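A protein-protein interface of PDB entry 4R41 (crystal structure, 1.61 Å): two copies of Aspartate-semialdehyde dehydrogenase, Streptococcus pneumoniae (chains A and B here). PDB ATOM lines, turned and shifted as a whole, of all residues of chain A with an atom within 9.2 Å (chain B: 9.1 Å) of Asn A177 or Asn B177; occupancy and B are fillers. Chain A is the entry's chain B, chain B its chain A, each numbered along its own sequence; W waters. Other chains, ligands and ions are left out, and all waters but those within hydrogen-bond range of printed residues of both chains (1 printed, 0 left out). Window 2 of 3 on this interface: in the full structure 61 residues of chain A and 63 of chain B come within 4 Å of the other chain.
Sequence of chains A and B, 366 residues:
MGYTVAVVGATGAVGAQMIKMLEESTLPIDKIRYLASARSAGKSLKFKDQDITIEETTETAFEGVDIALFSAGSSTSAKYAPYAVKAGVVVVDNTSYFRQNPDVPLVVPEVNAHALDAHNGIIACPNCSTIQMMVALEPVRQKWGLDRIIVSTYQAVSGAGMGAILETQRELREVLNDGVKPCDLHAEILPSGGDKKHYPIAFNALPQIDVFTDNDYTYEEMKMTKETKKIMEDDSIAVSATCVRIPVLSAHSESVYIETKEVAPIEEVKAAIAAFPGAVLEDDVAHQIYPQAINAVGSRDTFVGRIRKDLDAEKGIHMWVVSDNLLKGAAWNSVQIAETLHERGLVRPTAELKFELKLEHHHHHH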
ATOM      1  N   GLN A 169     -10.424 -19.402   2.275  1.00  0.00           N
ATOM      2  CA  GLN A 169     -11.273 -19.549   3.463  1.00  0.00           C
ATOM      3  C   GLN A 169     -10.459 -19.682   4.745  1.00  0.00           C
ATOM      4  O   GLN A 169     -10.774 -19.059   5.750  1.00  0.00           O
ATOM      5  CB  GLN A 169     -12.222 -20.747   3.299  1.00  0.00           C
ATOM      6  CG  GLN A 169     -13.333 -20.470   2.286  1.00  0.00           C
ATOM      7  CD  GLN A 169     -14.071 -21.736   1.851  1.00  0.00           C
ATOM      8  OE1 GLN A 169     -13.464 -22.793   1.621  1.00  0.00           O
ATOM      9  NE2 GLN A 169     -15.390 -21.631   1.744  1.00  0.00           N
ATOM     10  N   ARG A 170      -9.413 -20.503   4.701  1.00  0.00           N
ATOM     11  CA  ARG A 170      -8.551 -20.692   5.882  1.00  0.00           C
ATOM     12  C   ARG A 170      -7.871 -19.371   6.286  1.00  0.00           C
ATOM     13  O   ARG A 170      -7.885 -18.993   7.467  1.00  0.00           O
ATOM     14  CB  ARG A 170      -7.526 -21.800   5.629  1.00  0.00           C
ATOM     15  CG  ARG A 170      -6.667 -22.148   6.850  1.00  0.00           C
ATOM     16  CD  ARG A 170      -5.342 -21.400   6.855  1.00  0.00           C
ATOM     17  NE  ARG A 170      -4.557 -21.621   5.636  1.00  0.00           N
ATOM     18  CZ  ARG A 170      -3.541 -20.843   5.258  1.00  0.00           C
ATOM     19  NH1 ARG A 170      -3.188 -19.798   5.995  1.00  0.00           N
ATOM     20  NH2 ARG A 170      -2.885 -21.095   4.139  1.00  0.00           N
ATOM     21  N   GLU A 171      -7.307 -18.659   5.301  1.00  0.00           N
ATOM     22  CA  GLU A 171      -6.672 -17.361   5.567  1.00  0.00           C
ATOM     23  C   GLU A 171      -7.658 -16.397   6.231  1.00  0.00           C
ATOM     24  O   GLU A 171      -7.332 -15.789   7.251  1.00  0.00           O
ATOM     25  CB  GLU A 171      -6.103 -16.736   4.280  1.00  0.00           C
ATOM     26  CG  GLU A 171      -4.835 -17.397   3.771  1.00  0.00           C
ATOM     27  CD  GLU A 171      -4.383 -16.848   2.431  1.00  0.00           C
ATOM     28  OE1 GLU A 171      -4.925 -15.785   2.025  1.00  0.00           O
ATOM     29  OE2 GLU A 171      -3.456 -17.467   1.808  1.00  0.00           O
ATOM     30  N   LEU A 172      -8.863 -16.256   5.664  1.00  0.00           N
ATOM     31  CA  LEU A 172      -9.839 -15.313   6.238  1.00  0.00           C
ATOM     32  C   LEU A 172     -10.207 -15.671   7.690  1.00  0.00           C
ATOM     33  O   LEU A 172     -10.350 -14.799   8.531  1.00  0.00           O
ATOM     34  CB  LEU A 172     -11.110 -15.246   5.388  1.00  0.00           C
ATOM     35  CG  LEU A 172     -10.967 -14.562   4.025  1.00  0.00           C
ATOM     36  CD1 LEU A 172     -12.130 -14.962   3.138  1.00  0.00           C
ATOM     37  CD2 LEU A 172     -10.886 -13.059   4.207  1.00  0.00           C
ATOM     38  N   ARG A 173     -10.366 -16.961   7.970  1.00  0.00           N
ATOM     39  CA  ARG A 173     -10.663 -17.392   9.335  1.00  0.00           C
ATOM     40  C   ARG A 173      -9.502 -17.090  10.271  1.00  0.00           C
ATOM     41  O   ARG A 173      -9.718 -16.691  11.407  1.00  0.00           O
ATOM     42  CB  ARG A 173     -11.031 -18.880   9.380  1.00  0.00           C
ATOM     43  CG  ARG A 173     -12.438 -19.176   8.877  1.00  0.00           C
ATOM     44  CD  ARG A 173     -12.814 -20.619   9.164  1.00  0.00           C
ATOM     45  NE  ARG A 173     -11.682 -21.511   8.930  1.00  0.00           N
ATOM     46  CZ  ARG A 173     -11.537 -22.297   7.868  1.00  0.00           C
ATOM     47  NH1 ARG A 173     -12.465 -22.327   6.919  1.00  0.00           N
ATOM     48  NH2 ARG A 173     -10.461 -23.062   7.762  1.00  0.00           N
ATOM     49  N   GLU A 174      -8.272 -17.272   9.797  1.00  0.00           N
ATOM     50  CA  GLU A 174      -7.110 -16.919  10.650  1.00  0.00           C
ATOM     51  C   GLU A 174      -7.100 -15.451  11.079  1.00  0.00           C
ATOM     52  O   GLU A 174      -6.810 -15.113  12.233  1.00  0.00           O
ATOM     53  CB  GLU A 174      -5.800 -17.318   9.989  1.00  0.00           C
ATOM     54  CG  GLU A 174      -5.593 -18.822  10.041  1.00  0.00           C
ATOM     55  CD  GLU A 174      -4.236 -19.275   9.546  1.00  0.00           C
ATOM     56  OE1 GLU A 174      -3.667 -20.209  10.162  1.00  0.00           O
ATOM     57  OE2 GLU A 174      -3.737 -18.736   8.551  1.00  0.00           O
ATOM     58  N   VAL A 175      -7.438 -14.582  10.138  1.00  0.00           N
ATOM     59  CA  VAL A 175      -7.515 -13.155  10.417  1.00  0.00           C
ATOM     60  C   VAL A 175      -8.669 -12.819  11.380  1.00  0.00           C
ATOM     61  O   VAL A 175      -8.476 -12.128  12.371  1.00  0.00           O
ATOM     62  CB  VAL A 175      -7.646 -12.345   9.100  1.00  0.00           C
ATOM     63  CG1 VAL A 175      -7.743 -10.851   9.392  1.00  0.00           C
ATOM     64  CG2 VAL A 175      -6.457 -12.627   8.194  1.00  0.00           C
ATOM     65  N   LEU A 176      -9.860 -13.329  11.095  1.00  0.00           N
ATOM     66  CA  LEU A 176     -11.068 -12.874  11.763  1.00  0.00           C
ATOM     67  C   LEU A 176     -11.258 -13.566  13.110  1.00  0.00           C
ATOM     68  O   LEU A 176     -11.784 -12.965  14.056  1.00  0.00           O
ATOM     69  CB  LEU A 176     -12.285 -13.116  10.864  1.00  0.00           C
ATOM     70  CG  LEU A 176     -12.360 -12.152   9.676  1.00  0.00           C
ATOM     71  CD1 LEU A 176     -13.182 -12.779   8.561  1.00  0.00           C
ATOM     72  CD2 LEU A 176     -12.950 -10.818  10.118  1.00  0.00           C
ATOM     73  N   ASN A 177     -10.803 -14.814  13.188  1.00  0.00           N
ATOM     74  CA  ASN A 177     -10.986 -15.632  14.380  1.00  0.00           C
ATOM     75  C   ASN A 177      -9.771 -15.638  15.301  1.00  0.00           C
ATOM     76  O   ASN A 177      -9.929 -15.662  16.521  1.00  0.00           O
ATOM     77  CB  ASN A 177     -11.359 -17.066  13.992  1.00  0.00           C
ATOM     78  CG  ASN A 177     -12.694 -17.154  13.282  1.00  0.00           C
ATOM     79  OD1 ASN A 177     -13.515 -16.247  13.378  1.00  0.00           O
ATOM     80  ND2 ASN A 177     -12.932 -18.264  12.582  1.00  0.00           N
ATOM     81  N   ASP A 178      -8.570 -15.638  14.721  1.00  0.00           N
ATOM     82  CA  ASP A 178      -7.322 -15.698  15.501  1.00  0.00           C
ATOM     83  C   ASP A 178      -6.594 -14.361  15.636  1.00  0.00           C
ATOM     84  O   ASP A 178      -5.638 -14.241  16.411  1.00  0.00           O
ATOM     85  CB  ASP A 178      -6.361 -16.722  14.890  1.00  0.00           C
ATOM     86  CG  ASP A 178      -6.866 -18.155  15.008  1.00  0.00           C
ATOM     87  OD1 ASP A 178      -7.618 -18.439  15.955  1.00  0.00           O
ATOM     88  OD2 ASP A 178      -6.478 -19.002  14.163  1.00  0.00           O
ATOM     89  N   GLY A 179      -7.026 -13.362  14.876  1.00  0.00           N
ATOM     90  CA  GLY A 179      -6.386 -12.049  14.920  1.00  0.00           C
ATOM     91  C   GLY A 179      -5.036 -11.957  14.229  1.00  0.00           C
ATOM     92  O   GLY A 179      -4.254 -11.060  14.542  1.00  0.00           O
ATOM     93  N   VAL A 180      -4.755 -12.856  13.281  1.00  0.00           N
ATOM     94  CA  VAL A 180      -3.509 -12.810  12.504  1.00  0.00           C
ATOM     95  C   VAL A 180      -3.558 -11.623  11.528  1.00  0.00           C
ATOM     96  O   VAL A 180      -4.553 -11.435  10.842  1.00  0.00           O
ATOM     97  CB  VAL A 180      -3.265 -14.136  11.722  1.00  0.00           C
ATOM     98  CG1 VAL A 180      -2.008 -14.074  10.879  1.00  0.00           C
ATOM     99  CG2 VAL A 180      -3.178 -15.348  12.652  1.00  0.00           C
ATOM    100  N   PHE A 203      -8.192 -10.198   2.493  1.00  0.00           N
ATOM    101  CA  PHE A 203      -8.149  -8.730   2.614  1.00  0.00           C
ATOM    102  C   PHE A 203      -7.118  -8.081   1.672  1.00  0.00           C
ATOM    103  O   PHE A 203      -6.513  -7.055   1.997  1.00  0.00           O
ATOM    104  CB  PHE A 203      -7.936  -8.315   4.085  1.00  0.00           C
ATOM    105  CG  PHE A 203      -8.991  -8.837   4.990  1.00  0.00           C
ATOM    106  CD1 PHE A 203     -10.227  -8.208   5.069  1.00  0.00           C
ATOM    107  CD2 PHE A 203      -8.771 -10.016   5.728  1.00  0.00           C
ATOM    108  CE1 PHE A 203     -11.222  -8.699   5.909  1.00  0.00           C
ATOM    109  CE2 PHE A 203      -9.763 -10.515   6.558  1.00  0.00           C
ATOM    110  CZ  PHE A 203     -10.988  -9.849   6.655  1.00  0.00           C
ATOM    111  N   GLN B 169     -16.642  -7.179   8.834  1.00  0.00           N
ATOM    112  CA  GLN B 169     -16.180  -8.240   9.740  1.00  0.00           C
ATOM    113  C   GLN B 169     -17.321  -9.178  10.145  1.00  0.00           C
ATOM    114  O   GLN B 169     -17.176 -10.402  10.117  1.00  0.00           O
ATOM    115  CB  GLN B 169     -15.529  -7.635  10.980  1.00  0.00           C
ATOM    116  CG  GLN B 169     -14.198  -6.947  10.680  1.00  0.00           C
ATOM    117  CD  GLN B 169     -13.631  -6.184  11.868  1.00  0.00           C
ATOM    118  OE1 GLN B 169     -14.362  -5.562  12.640  1.00  0.00           O
ATOM    119  NE2 GLN B 169     -12.315  -6.225  12.011  1.00  0.00           N
ATOM    120  N   ARG B 170     -18.458  -8.592  10.510  1.00  0.00           N
ATOM    121  CA  ARG B 170     -19.630  -9.379  10.912  1.00  0.00           C
ATOM    122  C   ARG B 170     -20.096 -10.287   9.782  1.00  0.00           C
ATOM    123  O   ARG B 170     -20.308 -11.484   9.991  1.00  0.00           O
ATOM    124  CB  ARG B 170     -20.767  -8.448  11.365  1.00  0.00           C
ATOM    125  CG  ARG B 170     -21.911  -9.158  12.090  1.00  0.00           C
ATOM    126  CD  ARG B 170     -23.180  -9.241  11.252  1.00  0.00           C
ATOM    127  NE  ARG B 170     -23.562  -7.983  10.594  1.00  0.00           N
ATOM    128  CZ  ARG B 170     -24.294  -7.928   9.487  1.00  0.00           C
ATOM    129  NH1 ARG B 170     -24.749  -9.044   8.931  1.00  0.00           N
ATOM    130  NH2 ARG B 170     -24.592  -6.756   8.940  1.00  0.00           N
ATOM    131  N   GLU B 171     -20.274  -9.713   8.587  1.00  0.00           N
ATOM    132  CA  GLU B 171     -20.709 -10.497   7.427  1.00  0.00           C
ATOM    133  C   GLU B 171     -19.756 -11.661   7.118  1.00  0.00           C
ATOM    134  O   GLU B 171     -20.197 -12.797   6.881  1.00  0.00           O
ATOM    135  CB  GLU B 171     -20.857  -9.605   6.194  1.00  0.00           C
ATOM    136  CG  GLU B 171     -22.061  -8.684   6.248  1.00  0.00           C
ATOM    137  CD  GLU B 171     -22.114  -7.704   5.086  1.00  0.00           C
ATOM    138  OE1 GLU B 171     -21.381  -7.903   4.101  1.00  0.00           O
ATOM    139  OE2 GLU B 171     -22.909  -6.734   5.176  1.00  0.00           O
ATOM    140  N   LEU B 172     -18.455 -11.388   7.106  1.00  0.00           N
ATOM    141  CA  LEU B 172     -17.483 -12.433   6.792  1.00  0.00           C
ATOM    142  C   LEU B 172     -17.555 -13.557   7.828  1.00  0.00           C
ATOM    143  O   LEU B 172     -17.467 -14.737   7.473  1.00  0.00           O
ATOM    144  CB  LEU B 172     -16.061 -11.857   6.716  1.00  0.00           C
ATOM    145  CG  LEU B 172     -15.768 -11.036   5.448  1.00  0.00           C
ATOM    146  CD1 LEU B 172     -14.540 -10.154   5.615  1.00  0.00           C
ATOM    147  CD2 LEU B 172     -15.629 -11.945   4.235  1.00  0.00           C
ATOM    148  N   ARG B 173     -17.739 -13.194   9.092  1.00  0.00           N
ATOM    149  CA  ARG B 173     -17.820 -14.227  10.151  1.00  0.00           C
ATOM    150  C   ARG B 173     -19.081 -15.070   9.997  1.00  0.00           C
ATOM    151  O   ARG B 173     -19.050 -16.281  10.164  1.00  0.00           O
ATOM    152  CB  ARG B 173     -17.729 -13.619  11.567  1.00  0.00           C
ATOM    153  CG  ARG B 173     -16.327 -13.155  11.947  1.00  0.00           C
ATOM    154  CD  ARG B 173     -16.301 -12.536  13.348  1.00  0.00           C
ATOM    155  NE  ARG B 173     -14.977 -12.045  13.692  1.00  0.00           N
ATOM    156  CZ  ARG B 173     -14.680 -10.778  13.978  1.00  0.00           C
ATOM    157  NH1 ARG B 173     -15.624  -9.845  13.993  1.00  0.00           N
ATOM    158  NH2 ARG B 173     -13.433 -10.453  14.277  1.00  0.00           N
ATOM    159  N   GLU B 174     -20.191 -14.426   9.659  1.00  0.00           N
ATOM    160  CA  GLU B 174     -21.448 -15.146   9.435  1.00  0.00           C
ATOM    161  C   GLU B 174     -21.303 -16.183   8.333  1.00  0.00           C
ATOM    162  O   GLU B 174     -21.774 -17.316   8.473  1.00  0.00           O
ATOM    163  CB  GLU B 174     -22.607 -14.175   9.143  1.00  0.00           C
ATOM    164  CG  GLU B 174     -23.114 -13.482  10.402  1.00  0.00           C
ATOM    165  CD  GLU B 174     -24.070 -12.343  10.135  1.00  0.00           C
ATOM    166  OE1 GLU B 174     -24.608 -11.786  11.109  1.00  0.00           O
ATOM    167  OE2 GLU B 174     -24.282 -11.968   8.966  1.00  0.00           O
ATOM    168  N   VAL B 175     -20.648 -15.810   7.236  1.00  0.00           N
ATOM    169  CA  VAL B 175     -20.438 -16.748   6.143  1.00  0.00           C
ATOM    170  C   VAL B 175     -19.493 -17.865   6.562  1.00  0.00           C
ATOM    171  O   VAL B 175     -19.813 -19.050   6.385  1.00  0.00           O
ATOM    172  CB  VAL B 175     -19.892 -16.056   4.864  1.00  0.00           C
ATOM    173  CG1 VAL B 175     -19.706 -17.080   3.757  1.00  0.00           C
ATOM    174  CG2 VAL B 175     -20.887 -15.018   4.385  1.00  0.00           C
ATOM    175  N   LEU B 176     -18.343 -17.492   7.120  1.00  0.00           N
ATOM    176  CA  LEU B 176     -17.249 -18.447   7.340  1.00  0.00           C
ATOM    177  C   LEU B 176     -17.437 -19.303   8.584  1.00  0.00           C
ATOM    178  O   LEU B 176     -16.965 -20.442   8.618  1.00  0.00           O
ATOM    179  CB  LEU B 176     -15.933 -17.697   7.447  1.00  0.00           C
ATOM    180  CG  LEU B 176     -15.501 -17.106   6.102  1.00  0.00           C
ATOM    181  CD1 LEU B 176     -14.484 -16.017   6.364  1.00  0.00           C
ATOM    182  CD2 LEU B 176     -14.948 -18.197   5.190  1.00  0.00           C
ATOM    183  N   ASN B 177     -18.080 -18.741   9.603  1.00  0.00           N
ATOM    184  CA  ASN B 177     -18.269 -19.444  10.880  1.00  0.00           C
ATOM    185  C   ASN B 177     -19.678 -20.019  11.025  1.00  0.00           C
ATOM    186  O   ASN B 177     -19.850 -21.077  11.625  1.00  0.00           O
ATOM    187  CB  ASN B 177     -17.945 -18.544  12.079  1.00  0.00           C
ATOM    188  CG  ASN B 177     -16.498 -18.053  12.080  1.00  0.00           C
ATOM    189  OD1 ASN B 177     -15.600 -18.679  11.498  1.00  0.00           O
ATOM    190  ND2 ASN B 177     -16.271 -16.924  12.722  1.00  0.00           N
ATOM    191  N   ASP B 178     -20.680 -19.323  10.488  1.00  0.00           N
ATOM    192  CA  ASP B 178     -22.079 -19.757  10.663  1.00  0.00           C
ATOM    193  C   ASP B 178     -22.672 -20.439   9.436  1.00  0.00           C
ATOM    194  O   ASP B 178     -23.776 -20.990   9.495  1.00  0.00           O
ATOM    195  CB  ASP B 178     -22.985 -18.591  11.111  1.00  0.00           C
ATOM    196  CG  ASP B 178     -22.622 -18.046  12.477  1.00  0.00           C
ATOM    197  OD1 ASP B 178     -22.007 -18.770  13.290  1.00  0.00           O
ATOM    198  OD2 ASP B 178     -22.947 -16.865  12.742  1.00  0.00           O
ATOM    199  N   GLY B 179     -21.951 -20.396   8.318  1.00  0.00           N
ATOM    200  CA  GLY B 179     -22.429 -20.986   7.076  1.00  0.00           C
ATOM    201  C   GLY B 179     -23.557 -20.227   6.400  1.00  0.00           C
ATOM    202  O   GLY B 179     -24.302 -20.796   5.615  1.00  0.00           O
ATOM    203  N   VAL B 180     -23.671 -18.931   6.677  1.00  0.00           N
ATOM    204  CA  VAL B 180     -24.632 -18.078   5.951  1.00  0.00           C
ATOM    205  C   VAL B 180     -24.175 -17.874   4.498  1.00  0.00           C
ATOM    206  O   VAL B 180     -23.009 -17.577   4.261  1.00  0.00           O
ATOM    207  CB  VAL B 180     -24.824 -16.711   6.673  1.00  0.00           C
ATOM    208  CG1 VAL B 180     -25.859 -15.848   5.958  1.00  0.00           C
ATOM    209  CG2 VAL B 180     -25.218 -16.906   8.137  1.00  0.00           C
ATOM    210  N   PHE B 203     -17.378 -11.320   0.187  1.00  0.00           N
ATOM    211  CA  PHE B 203     -17.206 -12.084  -1.041  1.00  0.00           C
ATOM    212  C   PHE B 203     -17.916 -11.435  -2.238  1.00  0.00           C
ATOM    213  O   PHE B 203     -18.418 -12.124  -3.122  1.00  0.00           O
ATOM    214  CB  PHE B 203     -17.683 -13.523  -0.832  1.00  0.00           C
ATOM    215  CG  PHE B 203     -16.978 -14.219   0.290  1.00  0.00           C
ATOM    216  CD1 PHE B 203     -15.685 -14.696   0.117  1.00  0.00           C
ATOM    217  CD2 PHE B 203     -17.595 -14.364   1.522  1.00  0.00           C
ATOM    218  CE1 PHE B 203     -15.019 -15.349   1.153  1.00  0.00           C
ATOM    219  CE2 PHE B 203     -16.934 -15.007   2.569  1.00  0.00           C
ATOM    220  CZ  PHE B 203     -15.647 -15.500   2.378  1.00  0.00           C
HETATM  221  O   HOH W   1     -14.457 -14.493  15.316  1.00  0.00           O
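Water W1 lies within hydrogen-bond range of the side-chain amide oxygen (OD1) of Asn A177 (2.8 Å), the guanidinium group (NE) of Arg B173 (3.0 Å) and the backbone carbonyl oxygen (O) of Leu A176 (3.3 Å).
Of the printed residues of chain B, Asn A177 touches Asn B177 (2.9 Å).
Asn B177 touches one residue of chain A.
Printed residues of chain A within 4 Å of Leu B176: Leu A172.
Printed residues of chain A within 4 Å of Leu B172: Leu A176 and Phe A203.
Gly B179 touches none of the printed residues of chain A.
Val A175 touches none of the printed residues of chain B.
N of Asp B178 is in hydrogen-bond range of O of Arg B173 (3.5 Å).
ND2 of Asn A177 sits at hydrogen-bond distance from OD1 of Asn B177 (2.9 Å).
The guanidinium group of Arg B173 lies within hydrogen-bond range of the backbone carbonyl oxygen of Leu A176 (3.0 Å).
Among the printed residues, merely in contact across the chains: Leu A172 with Leu B176 (3.6 Å), Leu A172 with Phe B203 (3.5 Å), Leu A176 with Leu B172 (3.5 Å) and Phe A203 with Leu B172 (3.6 Å).
Leu A172 touches Leu B176, and with the chains exchanged Leu A176 touches Leu B172.
Leu A172 touches Phe B203, and with the chains exchanged Phe A203 touches Leu B172.
Leu A176 touches Arg B173, but with the chains exchanged Arg A173 does not touch Leu B176 (4.1 Å).
Asn A177 touches its own counterpart, Asn B177.
Positions printed for both chains: 169, 170, 171, 172, 173, 174, 175, 176, 177, 178, 179, 180 and 203.
Of the 13 printed residues of chain B, 5 touch a printed residue of chain A.
Hydrophobic or aromatic side chains of chain B within 4 Å of the printed part of chain A: Leu B172, Leu B176 and Phe B203.
Hydrophobic or aromatic side chains of chain A within 4 Å of the printed part of chain B: Leu A172, Leu A176 and Phe A203.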
